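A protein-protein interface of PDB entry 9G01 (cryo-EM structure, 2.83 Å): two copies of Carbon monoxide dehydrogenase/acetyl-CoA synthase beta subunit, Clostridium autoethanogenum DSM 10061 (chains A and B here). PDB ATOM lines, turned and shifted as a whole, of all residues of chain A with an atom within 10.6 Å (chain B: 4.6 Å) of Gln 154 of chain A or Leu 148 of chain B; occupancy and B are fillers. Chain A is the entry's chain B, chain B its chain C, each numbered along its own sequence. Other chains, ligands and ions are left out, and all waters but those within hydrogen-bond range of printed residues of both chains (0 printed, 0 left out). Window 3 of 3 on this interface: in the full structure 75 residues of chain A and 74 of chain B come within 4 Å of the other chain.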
ATOM      1  N   ARG A  97     -23.391  38.555  -8.354  1.00  0.00           N
ATOM      2  CA  ARG A  97     -22.076  38.948  -8.857  1.00  0.00           C
ATOM      3  C   ARG A  97     -21.927  40.464  -8.891  1.00  0.00           C
ATOM      4  O   ARG A  97     -20.880  41.000  -8.503  1.00  0.00           O
ATOM      5  CB  ARG A  97     -21.853  38.352 -10.251  1.00  0.00           C
ATOM      6  CG  ARG A  97     -20.409  38.514 -10.781  1.00  0.00           C
ATOM      7  CD  ARG A  97     -20.378  38.625 -12.327  1.00  0.00           C
ATOM      8  NE  ARG A  97     -21.332  37.706 -12.946  1.00  0.00           N
ATOM      9  CZ  ARG A  97     -21.158  36.395 -13.057  1.00  0.00           C
ATOM     10  NH1 ARG A  97     -20.053  35.804 -12.639  1.00  0.00           N
ATOM     11  NH2 ARG A  97     -22.127  35.651 -13.590  1.00  0.00           N
ATOM     12  N   LEU A 148     -16.481  36.385  -4.920  1.00  0.00           N
ATOM     13  CA  LEU A 148     -16.279  36.305  -6.365  1.00  0.00           C
ATOM     14  C   LEU A 148     -15.674  34.967  -6.761  1.00  0.00           C
ATOM     15  O   LEU A 148     -16.059  34.381  -7.779  1.00  0.00           O
ATOM     16  CB  LEU A 148     -15.392  37.458  -6.850  1.00  0.00           C
ATOM     17  CG  LEU A 148     -16.065  38.840  -6.856  1.00  0.00           C
ATOM     18  CD1 LEU A 148     -15.033  39.941  -7.081  1.00  0.00           C
ATOM     19  CD2 LEU A 148     -17.181  38.922  -7.909  1.00  0.00           C
ATOM     20  N   SER A 149     -14.743  34.448  -5.958  1.00  0.00           N
ATOM     21  CA  SER A 149     -14.175  33.141  -6.265  1.00  0.00           C
ATOM     22  C   SER A 149     -15.253  32.058  -6.226  1.00  0.00           C
ATOM     23  O   SER A 149     -15.198  31.108  -7.013  1.00  0.00           O
ATOM     24  CB  SER A 149     -13.003  32.818  -5.320  1.00  0.00           C
ATOM     25  OG  SER A 149     -13.428  32.425  -4.023  1.00  0.00           O
ATOM     26  N   ASN A 150     -16.279  32.219  -5.378  1.00  0.00           N
ATOM     27  CA  ASN A 150     -17.385  31.255  -5.391  1.00  0.00           C
ATOM     28  C   ASN A 150     -18.037  31.149  -6.773  1.00  0.00           C
ATOM     29  O   ASN A 150     -18.609  30.105  -7.104  1.00  0.00           O
ATOM     30  CB  ASN A 150     -18.458  31.622  -4.352  1.00  0.00           C
ATOM     31  CG  ASN A 150     -18.358  30.796  -3.068  1.00  0.00           C
ATOM     32  OD1 ASN A 150     -17.480  29.950  -2.943  1.00  0.00           O
ATOM     33  ND2 ASN A 150     -19.254  31.051  -2.108  1.00  0.00           N
ATOM     34  N   TYR A 151     -17.994  32.211  -7.581  1.00  0.00           N
ATOM     35  CA  TYR A 151     -18.671  32.166  -8.876  1.00  0.00           C
ATOM     36  C   TYR A 151     -17.899  31.387  -9.933  1.00  0.00           C
ATOM     37  O   TYR A 151     -18.522  30.754 -10.793  1.00  0.00           O
ATOM     38  CB  TYR A 151     -18.934  33.587  -9.392  1.00  0.00           C
ATOM     39  CG  TYR A 151     -20.064  34.256  -8.653  1.00  0.00           C
ATOM     40  CD1 TYR A 151     -19.825  34.966  -7.470  1.00  0.00           C
ATOM     41  CD2 TYR A 151     -21.384  34.153  -9.112  1.00  0.00           C
ATOM     42  CE1 TYR A 151     -20.868  35.575  -6.767  1.00  0.00           C
ATOM     43  CE2 TYR A 151     -22.444  34.759  -8.414  1.00  0.00           C
ATOM     44  CZ  TYR A 151     -22.169  35.466  -7.243  1.00  0.00           C
ATOM     45  OH  TYR A 151     -23.172  36.075  -6.522  1.00  0.00           O
ATOM     46  N   GLY A 152     -16.567  31.433  -9.917  1.00  0.00           N
ATOM     47  CA  GLY A 152     -15.820  30.901 -11.042  1.00  0.00           C
ATOM     48  C   GLY A 152     -14.582  30.084 -10.725  1.00  0.00           C
ATOM     49  O   GLY A 152     -13.766  29.850 -11.620  1.00  0.00           O
ATOM     50  N   LYS A 153     -14.430  29.619  -9.487  1.00  0.00           N
ATOM     51  CA  LYS A 153     -13.288  28.779  -9.144  1.00  0.00           C
ATOM     52  C   LYS A 153     -13.383  27.436  -9.862  1.00  0.00           C
ATOM     53  O   LYS A 153     -14.451  26.821  -9.922  1.00  0.00           O
ATOM     54  CB  LYS A 153     -13.197  28.576  -7.626  1.00  0.00           C
ATOM     55  CG  LYS A 153     -14.416  27.871  -7.003  1.00  0.00           C
ATOM     56  CD  LYS A 153     -13.983  26.925  -5.870  1.00  0.00           C
ATOM     57  CE  LYS A 153     -13.209  27.670  -4.770  1.00  0.00           C
ATOM     58  NZ  LYS A 153     -14.038  28.786  -4.176  1.00  0.00           N
ATOM     59  N   GLN A 154     -12.251  26.974 -10.402  1.00  0.00           N
ATOM     60  CA  GLN A 154     -12.179  25.702 -11.113  1.00  0.00           C
ATOM     61  C   GLN A 154     -11.505  24.600 -10.307  1.00  0.00           C
ATOM     62  O   GLN A 154     -11.682  23.421 -10.627  1.00  0.00           O
ATOM     63  CB  GLN A 154     -11.430  25.885 -12.448  1.00  0.00           C
ATOM     64  CG  GLN A 154     -12.022  27.007 -13.323  1.00  0.00           C
ATOM     65  CD  GLN A 154     -13.474  26.732 -13.718  1.00  0.00           C
ATOM     66  OE1 GLN A 154     -13.794  25.648 -14.198  1.00  0.00           O
ATOM     67  NE2 GLN A 154     -14.358  27.710 -13.509  1.00  0.00           N
ATOM     68  N   LEU A 155     -10.768  24.958  -9.261  1.00  0.00           N
ATOM     69  CA  LEU A 155     -10.133  24.010  -8.362  1.00  0.00           C
ATOM     70  C   LEU A 155     -10.633  24.260  -6.946  1.00  0.00           C
ATOM     71  O   LEU A 155     -10.839  25.412  -6.548  1.00  0.00           O
ATOM     72  CB  LEU A 155      -8.600  24.137  -8.402  1.00  0.00           C
ATOM     73  CG  LEU A 155      -7.957  23.873  -9.772  1.00  0.00           C
ATOM     74  CD1 LEU A 155      -6.443  24.112  -9.733  1.00  0.00           C
ATOM     75  CD2 LEU A 155      -8.262  22.448 -10.253  1.00  0.00           C
ATOM     76  N   GLY A 156     -10.852  23.181  -6.200  1.00  0.00           N
ATOM     77  CA  GLY A 156     -11.278  23.291  -4.820  1.00  0.00           C
ATOM     78  C   GLY A 156     -12.782  23.316  -4.644  1.00  0.00           C
ATOM     79  O   GLY A 156     -13.571  23.227  -5.589  1.00  0.00           O
ATOM     80  N   GLU A 157     -13.178  23.446  -3.382  1.00  0.00           N
ATOM     81  CA  GLU A 157     -14.574  23.455  -2.983  1.00  0.00           C
ATOM     82  C   GLU A 157     -15.043  24.884  -2.731  1.00  0.00           C
ATOM     83  O   GLU A 157     -14.270  25.748  -2.310  1.00  0.00           O
ATOM     84  CB  GLU A 157     -14.782  22.600  -1.726  1.00  0.00           C
ATOM     85  CG  GLU A 157     -16.266  22.391  -1.367  1.00  0.00           C
ATOM     86  CD  GLU A 157     -16.475  22.134   0.116  1.00  0.00           C
ATOM     87  OE1 GLU A 157     -15.905  21.153   0.637  1.00  0.00           O
ATOM     88  OE2 GLU A 157     -17.192  22.926   0.765  1.00  0.00           O
ATOM     89  N   VAL A 158     -16.331  25.122  -2.989  1.00  0.00           N
ATOM     90  CA  VAL A 158     -16.955  26.422  -2.773  1.00  0.00           C
ATOM     91  C   VAL A 158     -17.210  26.639  -1.284  1.00  0.00           C
ATOM     92  O   VAL A 158     -17.101  25.704  -0.481  1.00  0.00           O
ATOM     93  CB  VAL A 158     -18.261  26.550  -3.583  1.00  0.00           C
ATOM     94  CG1 VAL A 158     -17.951  26.547  -5.091  1.00  0.00           C
ATOM     95  CG2 VAL A 158     -19.251  25.424  -3.236  1.00  0.00           C
ATOM     96  N   PRO A 179     -22.757  21.358  -4.717  1.00  0.00           N
ATOM     97  CA  PRO A 179     -22.511  22.434  -5.694  1.00  0.00           C
ATOM     98  C   PRO A 179     -21.038  22.720  -5.956  1.00  0.00           C
ATOM     99  O   PRO A 179     -20.174  22.558  -5.085  1.00  0.00           O
ATOM    100  CB  PRO A 179     -23.208  23.654  -5.065  1.00  0.00           C
ATOM    101  CG  PRO A 179     -23.224  23.354  -3.558  1.00  0.00           C
ATOM    102  CD  PRO A 179     -23.404  21.847  -3.481  1.00  0.00           C
ATOM    103  N   ARG A 180     -20.759  23.162  -7.189  1.00  0.00           N
ATOM    104  CA  ARG A 180     -19.499  23.745  -7.629  1.00  0.00           C
ATOM    105  C   ARG A 180     -19.736  25.243  -7.864  1.00  0.00           C
ATOM    106  O   ARG A 180     -20.785  25.786  -7.504  1.00  0.00           O
ATOM    107  CB  ARG A 180     -18.983  23.006  -8.876  1.00  0.00           C
ATOM    108  CG  ARG A 180     -18.699  21.503  -8.600  1.00  0.00           C
ATOM    109  CD  ARG A 180     -18.482  20.683  -9.888  1.00  0.00           C
ATOM    110  NE  ARG A 180     -19.637  20.724 -10.783  1.00  0.00           N
ATOM    111  CZ  ARG A 180     -19.719  20.069 -11.935  1.00  0.00           C
ATOM    112  NH1 ARG A 180     -18.741  19.288 -12.354  1.00  0.00           N
ATOM    113  NH2 ARG A 180     -20.810  20.208 -12.688  1.00  0.00           N
ATOM    114  N   ALA A 181     -18.753  25.912  -8.465  1.00  0.00           N
ATOM    115  CA  ALA A 181     -18.874  27.331  -8.790  1.00  0.00           C
ATOM    116  C   ALA A 181     -20.112  27.593  -9.648  1.00  0.00           C
ATOM    117  O   ALA A 181     -20.480  26.775 -10.499  1.00  0.00           O
ATOM    118  CB  ALA A 181     -17.604  27.817  -9.495  1.00  0.00           C
ATOM    119  N   VAL A 182     -20.768  28.737  -9.406  1.00  0.00           N
ATOM    120  CA  VAL A 182     -22.113  28.969  -9.941  1.00  0.00           C
ATOM    121  C   VAL A 182     -22.107  28.950 -11.468  1.00  0.00           C
ATOM    122  O   VAL A 182     -22.876  28.214 -12.108  1.00  0.00           O
ATOM    123  CB  VAL A 182     -22.670  30.315  -9.430  1.00  0.00           C
ATOM    124  CG1 VAL A 182     -24.117  30.506  -9.917  1.00  0.00           C
ATOM    125  CG2 VAL A 182     -22.586  30.455  -7.888  1.00  0.00           C
ATOM    126  N   ASP A 183     -21.217  29.739 -12.081  1.00  0.00           N
ATOM    127  CA  ASP A 183     -21.163  29.798 -13.540  1.00  0.00           C
ATOM    128  C   ASP A 183     -20.781  28.446 -14.132  1.00  0.00           C
ATOM    129  O   ASP A 183     -21.280  28.067 -15.197  1.00  0.00           O
ATOM    130  CB  ASP A 183     -20.184  30.886 -13.995  1.00  0.00           C
ATOM    131  CG  ASP A 183     -20.573  32.281 -13.515  1.00  0.00           C
ATOM    132  OD1 ASP A 183     -21.785  32.560 -13.373  1.00  0.00           O
ATOM    133  OD2 ASP A 183     -19.667  33.106 -13.288  1.00  0.00           O
ATOM    134  N   ARG A 184     -19.928  27.696 -13.434  1.00  0.00           N
ATOM    135  CA  ARG A 184     -19.574  26.351 -13.873  1.00  0.00           C
ATOM    136  C   ARG A 184     -20.803  25.446 -13.924  1.00  0.00           C
ATOM    137  O   ARG A 184     -20.974  24.682 -14.877  1.00  0.00           O
ATOM    138  CB  ARG A 184     -18.487  25.782 -12.952  1.00  0.00           C
ATOM    139  CG  ARG A 184     -17.717  24.584 -13.525  1.00  0.00           C
ATOM    140  CD  ARG A 184     -18.323  23.262 -13.039  1.00  0.00           C
ATOM    141  NE  ARG A 184     -17.724  22.117 -13.716  1.00  0.00           N
ATOM    142  CZ  ARG A 184     -18.002  21.750 -14.962  1.00  0.00           C
ATOM    143  NH1 ARG A 184     -18.881  22.407 -15.701  1.00  0.00           N
ATOM    144  NH2 ARG A 184     -17.369  20.701 -15.485  1.00  0.00           N
ATOM    145  N   GLU A 185     -21.691  25.535 -12.929  1.00  0.00           N
ATOM    146  CA  GLU A 185     -22.879  24.679 -12.924  1.00  0.00           C
ATOM    147  C   GLU A 185     -23.869  25.086 -14.012  1.00  0.00           C
ATOM    148  O   GLU A 185     -24.493  24.222 -14.652  1.00  0.00           O
ATOM    149  CB  GLU A 185     -23.547  24.713 -11.548  1.00  0.00           C
ATOM    150  CG  GLU A 185     -22.682  24.071 -10.452  1.00  0.00           C
ATOM    151  CD  GLU A 185     -22.486  22.571 -10.647  1.00  0.00           C
ATOM    152  OE1 GLU A 185     -23.019  22.014 -11.622  1.00  0.00           O
ATOM    153  OE2 GLU A 185     -21.794  21.944  -9.820  1.00  0.00           O
ATOM    154  N   ILE A 186     -24.023  26.391 -14.242  1.00  0.00           N
ATOM    155  CA  ILE A 186     -24.862  26.851 -15.350  1.00  0.00           C
ATOM    156  C   ILE A 186     -24.326  26.310 -16.673  1.00  0.00           C
ATOM    157  O   ILE A 186     -25.076  25.782 -17.511  1.00  0.00           O
ATOM    158  CB  ILE A 186     -24.947  28.390 -15.359  1.00  0.00           C
ATOM    159  CG1 ILE A 186     -25.643  28.903 -14.087  1.00  0.00           C
ATOM    160  CG2 ILE A 186     -25.662  28.895 -16.636  1.00  0.00           C
ATOM    161  CD1 ILE A 186     -25.471  30.399 -13.885  1.00  0.00           C
ATOM    162  N   ALA A 187     -23.010  26.416 -16.870  1.00  0.00           N
ATOM    163  CA  ALA A 187     -22.401  25.904 -18.097  1.00  0.00           C
ATOM    164  C   ALA A 187     -22.580  24.397 -18.217  1.00  0.00           C
ATOM    165  O   ALA A 187     -22.842  23.889 -19.308  1.00  0.00           O
ATOM    166  CB  ALA A 187     -20.917  26.278 -18.168  1.00  0.00           C
ATOM    167  N   ALA A 188     -22.470  23.668 -17.105  1.00  0.00           N
ATOM    168  CA  ALA A 188     -22.658  22.219 -17.143  1.00  0.00           C
ATOM    169  C   ALA A 188     -24.068  21.854 -17.588  1.00  0.00           C
ATOM    170  O   ALA A 188     -24.248  20.961 -18.425  1.00  0.00           O
ATOM    171  CB  ALA A 188     -22.371  21.603 -15.771  1.00  0.00           C
ATOM    172  N   ARG A 210     -28.364  20.327  -8.741  1.00  0.00           N
ATOM    173  CA  ARG A 210     -27.013  20.775  -8.434  1.00  0.00           C
ATOM    174  C   ARG A 210     -26.822  22.229  -8.839  1.00  0.00           C
ATOM    175  O   ARG A 210     -26.324  23.040  -8.051  1.00  0.00           O
ATOM    176  CB  ARG A 210     -26.000  19.869  -9.140  1.00  0.00           C
ATOM    177  CG  ARG A 210     -24.544  20.108  -8.738  1.00  0.00           C
ATOM    178  CD  ARG A 210     -23.619  19.180  -9.544  1.00  0.00           C
ATOM    179  NE  ARG A 210     -22.347  18.944  -8.871  1.00  0.00           N
ATOM    180  CZ  ARG A 210     -21.436  18.063  -9.265  1.00  0.00           C
ATOM    181  NH1 ARG A 210     -21.614  17.315 -10.338  1.00  0.00           N
ATOM    182  NH2 ARG A 210     -20.312  17.930  -8.557  1.00  0.00           N
ATOM    183  N   MET A 218     -25.435  30.068  -2.615  1.00  0.00           N
ATOM    184  CA  MET A 218     -24.268  30.879  -2.945  1.00  0.00           C
ATOM    185  C   MET A 218     -24.644  32.222  -3.559  1.00  0.00           C
ATOM    186  O   MET A 218     -24.342  33.266  -2.974  1.00  0.00           O
ATOM    187  CB  MET A 218     -23.345  30.082  -3.871  1.00  0.00           C
ATOM    188  CG  MET A 218     -23.023  28.698  -3.296  1.00  0.00           C
ATOM    189  SD  MET A 218     -22.228  27.637  -4.519  1.00  0.00           S
ATOM    190  CE  MET A 218     -20.831  28.653  -4.984  1.00  0.00           C
ATOM    191  N   ARG B  97     -12.457  22.827 -20.727  1.00  0.00           N
ATOM    192  CA  ARG B  97     -12.234  22.765 -19.285  1.00  0.00           C
ATOM    193  C   ARG B  97     -11.743  21.385 -18.863  1.00  0.00           C
ATOM    194  O   ARG B  97     -10.818  21.271 -18.048  1.00  0.00           O
ATOM    195  CB  ARG B  97     -13.525  23.123 -18.541  1.00  0.00           C
ATOM    196  CG  ARG B  97     -13.349  23.322 -17.015  1.00  0.00           C
ATOM    197  CD  ARG B  97     -14.642  22.958 -16.240  1.00  0.00           C
ATOM    198  NE  ARG B  97     -15.834  23.421 -16.948  1.00  0.00           N
ATOM    199  CZ  ARG B  97     -16.253  24.681 -16.984  1.00  0.00           C
ATOM    200  NH1 ARG B  97     -15.628  25.637 -16.323  1.00  0.00           N
ATOM    201  NH2 ARG B  97     -17.322  24.990 -17.716  1.00  0.00           N
ATOM    202  N   ALA B 100      -8.136  21.201 -19.837  1.00  0.00           N
ATOM    203  CA  ALA B 100      -7.274  21.974 -18.941  1.00  0.00           C
ATOM    204  C   ALA B 100      -7.066  21.248 -17.616  1.00  0.00           C
ATOM    205  O   ALA B 100      -5.951  21.231 -17.077  1.00  0.00           O
ATOM    206  CB  ALA B 100      -7.849  23.375 -18.716  1.00  0.00           C
ATOM    207  N   LEU B 101      -8.120  20.630 -17.074  1.00  0.00           N
ATOM    208  CA  LEU B 101      -7.963  19.853 -15.844  1.00  0.00           C
ATOM    209  C   LEU B 101      -7.023  18.666 -16.063  1.00  0.00           C
ATOM    210  O   LEU B 101      -6.154  18.381 -15.221  1.00  0.00           O
ATOM    211  CB  LEU B 101      -9.336  19.389 -15.328  1.00  0.00           C
ATOM    212  CG  LEU B 101     -10.256  20.529 -14.833  1.00  0.00           C
ATOM    213  CD1 LEU B 101     -11.675  20.027 -14.519  1.00  0.00           C
ATOM    214  CD2 LEU B 101      -9.674  21.253 -13.597  1.00  0.00           C
ATOM    215  N   ALA B 144      -1.794  25.217 -17.080  1.00  0.00           N
ATOM    216  CA  ALA B 144      -3.157  24.758 -16.827  1.00  0.00           C
ATOM    217  C   ALA B 144      -3.895  25.695 -15.879  1.00  0.00           C
ATOM    218  O   ALA B 144      -5.082  25.980 -16.078  1.00  0.00           O
ATOM    219  CB  ALA B 144      -3.141  23.327 -16.279  1.00  0.00           C
ATOM    220  N   LYS B 145      -3.205  26.215 -14.861  1.00  0.00           N
ATOM    221  CA  LYS B 145      -3.824  27.177 -13.949  1.00  0.00           C
ATOM    222  C   LYS B 145      -4.263  28.441 -14.683  1.00  0.00           C
ATOM    223  O   LYS B 145      -5.377  28.940 -14.470  1.00  0.00           O
ATOM    224  CB  LYS B 145      -2.868  27.531 -12.810  1.00  0.00           C
ATOM    225  CG  LYS B 145      -2.493  26.338 -11.932  1.00  0.00           C
ATOM    226  CD  LYS B 145      -1.134  26.597 -11.270  1.00  0.00           C
ATOM    227  CE  LYS B 145      -0.481  25.302 -10.780  1.00  0.00           C
ATOM    228  NZ  LYS B 145       0.978  25.509 -10.459  1.00  0.00           N
ATOM    229  N   GLU B 146      -3.405  28.973 -15.556  1.00  0.00           N
ATOM    230  CA  GLU B 146      -3.784  30.163 -16.322  1.00  0.00           C
ATOM    231  C   GLU B 146      -4.979  29.880 -17.230  1.00  0.00           C
ATOM    232  O   GLU B 146      -5.929  30.679 -17.309  1.00  0.00           O
ATOM    233  CB  GLU B 146      -2.596  30.655 -17.156  1.00  0.00           C
ATOM    234  CG  GLU B 146      -1.390  31.076 -16.323  1.00  0.00           C
ATOM    235  CD  GLU B 146      -1.743  32.180 -15.339  1.00  0.00           C
ATOM    236  OE1 GLU B 146      -2.429  33.138 -15.745  1.00  0.00           O
ATOM    237  OE2 GLU B 146      -1.357  32.080 -14.156  1.00  0.00           O
ATOM    238  N   GLY B 147      -4.964  28.726 -17.894  1.00  0.00           N
ATOM    239  CA  GLY B 147      -6.081  28.359 -18.748  1.00  0.00           C
ATOM    240  C   GLY B 147      -7.388  28.231 -17.985  1.00  0.00           C
ATOM    241  O   GLY B 147      -8.424  28.741 -18.415  1.00  0.00           O
ATOM    242  N   LEU B 148      -7.340  27.598 -16.811  1.00  0.00           N
ATOM    243  CA  LEU B 148      -8.529  27.472 -15.969  1.00  0.00           C
ATOM    244  C   LEU B 148      -9.025  28.833 -15.506  1.00  0.00           C
ATOM    245  O   LEU B 148     -10.235  29.080 -15.469  1.00  0.00           O
ATOM    246  CB  LEU B 148      -8.239  26.574 -14.760  1.00  0.00           C
ATOM    247  CG  LEU B 148      -8.088  25.077 -15.070  1.00  0.00           C
ATOM    248  CD1 LEU B 148      -7.505  24.337 -13.869  1.00  0.00           C
ATOM    249  CD2 LEU B 148      -9.425  24.453 -15.493  1.00  0.00           C
ATOM    250  N   SER B 149      -8.106  29.743 -15.181  1.00  0.00           N
ATOM    251  CA  SER B 149      -8.529  31.084 -14.789  1.00  0.00           C
ATOM    252  C   SER B 149      -9.261  31.776 -15.936  1.00  0.00           C
ATOM    253  O   SER B 149     -10.200  32.540 -15.694  1.00  0.00           O
ATOM    254  CB  SER B 149      -7.333  31.910 -14.285  1.00  0.00           C
ATOM    255  OG  SER B 149      -6.510  32.398 -15.335  1.00  0.00           O
ATOM    256  N   ASN B 150      -8.902  31.467 -17.190  1.00  0.00           N
ATOM    257  CA  ASN B 150      -9.658  32.032 -18.315  1.00  0.00           C
ATOM    258  C   ASN B 150     -11.145  31.680 -18.236  1.00  0.00           C
ATOM    259  O   ASN B 150     -11.981  32.415 -18.777  1.00  0.00           O
ATOM    260  CB  ASN B 150      -9.094  31.555 -19.664  1.00  0.00           C
ATOM    261  CG  ASN B 150      -8.195  32.593 -20.340  1.00  0.00           C
ATOM    262  OD1 ASN B 150      -7.970  33.667 -19.793  1.00  0.00           O
ATOM    263  ND2 ASN B 150      -7.674  32.266 -21.526  1.00  0.00           N
ATOM    264  N   TYR B 151     -11.503  30.554 -17.613  1.00  0.00           N
ATOM    265  CA  TYR B 151     -12.908  30.151 -17.598  1.00  0.00           C
ATOM    266  C   TYR B 151     -13.737  30.927 -16.580  1.00  0.00           C
ATOM    267  O   TYR B 151     -14.923  31.176 -16.831  1.00  0.00           O
ATOM    268  CB  TYR B 151     -13.033  28.650 -17.316  1.00  0.00           C
ATOM    269  CG  TYR B 151     -12.663  27.822 -18.519  1.00  0.00           C
ATOM    270  CD1 TYR B 151     -11.335  27.446 -18.748  1.00  0.00           C
ATOM    271  CD2 TYR B 151     -13.633  27.445 -19.457  1.00  0.00           C
ATOM    272  CE1 TYR B 151     -10.978  26.696 -19.871  1.00  0.00           C
ATOM    273  CE2 TYR B 151     -13.289  26.692 -20.592  1.00  0.00           C
ATOM    274  CZ  TYR B 151     -11.958  26.325 -20.784  1.00  0.00           C
ATOM    275  OH  TYR B 151     -11.572  25.587 -21.883  1.00  0.00           O
ATOM    276  N   GLY B 152     -13.166  31.288 -15.432  1.00  0.00           N
ATOM    277  CA  GLY B 152     -13.988  31.804 -14.353  1.00  0.00           C
ATOM    278  C   GLY B 152     -13.456  33.004 -13.590  1.00  0.00           C
ATOM    279  O   GLY B 152     -13.963  33.305 -12.507  1.00  0.00           O
ATOM    280  N   ASP B 183     -17.424  31.068 -18.726  1.00  0.00           N
ATOM    281  CA  ASP B 183     -18.642  30.759 -17.978  1.00  0.00           C
ATOM    282  C   ASP B 183     -19.405  32.027 -17.616  1.00  0.00           C
ATOM    283  O   ASP B 183     -20.640  32.032 -17.613  1.00  0.00           O
ATOM    284  CB  ASP B 183     -18.312  29.954 -16.717  1.00  0.00           C
ATOM    285  CG  ASP B 183     -17.615  28.630 -17.014  1.00  0.00           C
ATOM    286  OD1 ASP B 183     -17.886  28.022 -18.072  1.00  0.00           O
ATOM    287  OD2 ASP B 183     -16.801  28.189 -16.179  1.00  0.00           O
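The guanidinium group of Arg 97 of chain A lies within salt-bridge range of the side-chain carboxylate of Asp 183 of chain A (2.8 Å).
O of Tyr 151 of chain A is in hydrogen-bond range of N of Asp 183 of chain A (3.2 Å).
The backbone carbonyl oxygen (O) of Gly 152 of chain A lies within hydrogen-bond range of the side-chain amide nitrogen (NE2) of Gln 154 of chain A (2.9 Å).
The backbone NH (N) of Arg 97 of chain B is in hydrogen-bond range of the side-chain hydroxyl (OH) of Tyr 151 of chain B.
The side-chain carboxylate (OD2) of Asp 183 of chain B is in salt-bridge range of the guanidinium group (NH1) of Arg 97 of chain B, 2.8 Å away.
O of Tyr 151 of chain B lies within hydrogen-bond range of N of Asp 183 of chain B, at 3.1 Å.
Of the 13 printed residues of chain B, 5 touch a printed residue of chain A.
Printed residues of chain B that touch a printed residue of chain A: Arg 97, Leu 101, Leu 148, Gly 152 and Asp 183.
Hydrophobic or aromatic side chains of chain B that line the printed part of chain A: Leu 101 and Leu 148.
Of the 24 printed residues of chain A, 6 touch a printed residue of chain B.
Among the printed residues, 9 pairs touch across the chains.
Among the printed residues, no Asp or Glu carboxylate lies within 4 Å of a Lys or Arg side-chain nitrogen of the other chain.
Gly 152 of chain B touches its own counterpart, Gly 152 of chain A.
Asp 183 of chain A touches its own counterpart, Asp 183 of chain B.
Positions printed for both chains: 97, 148, 149, 150, 151, 152 and 183.
OE1 of Gln 154 of chain A sits at hydrogen-bond distance from NH1 of Arg 97 of chain B (2.8 Å).
NH1 of Arg 184 of chain A sits close to NE of Arg 97 of chain B (3.4 Å).
Gln 154 of chain A touches three residues of chain B.
Of the printed residues of chain A, Leu 148 of chain B touches Gln 154.
No residue of chain A comes within 4 Å of Gly 147 of chain B.
Ser 149 of chain B touches none of the printed residues of chain A.
Gly 152 of chain B touches just one residue of chain A: Gly 152 (3.4 Å).
Printed residues of chain A within 4 Å of Asp 183 of chain B: Gln 154 (3.7 Å), Asp 183 (3.4 Å) and Ala 187 (3.5 Å).
Of the printed residues of chain B, Asp 183 of chain A touches Asp 183.
Of the printed residues of chain B, Gly 152 of chain A touches Gly 152 (3.4 Å).
Of the printed residues of chain B, Arg 184 of chain A touches Arg 97 (3.4 Å).
Leu 148 of chain A touches none of the printed residues of chain B.
The nearest residue of chain B that does not touch Gln 154 of chain A is Tyr 151 of chain B (4.1 Å).
Gly 152 of chain A touches Gly 152 of chain B (O to CA, 3.4 Å).
O of Leu 148 of chain B touches CG of Gln 154 of chain A, at 3.5 Å.
OD2 of Asp 183 of chain B touches NE2 of Gln 154 of chain A, 3.7 Å away.
Leu 155 of chain A touches Leu 101 of chain B (CD2 to CD2, 3.8 Å).
Asp 183 of chain B touches Asp 183 of chain A.
Ala 187 of chain A touches Arg 97 of chain B.
Asp 183 of chain B touches Ala 187 of chain A (OD1 to CB, 3.5 Å).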
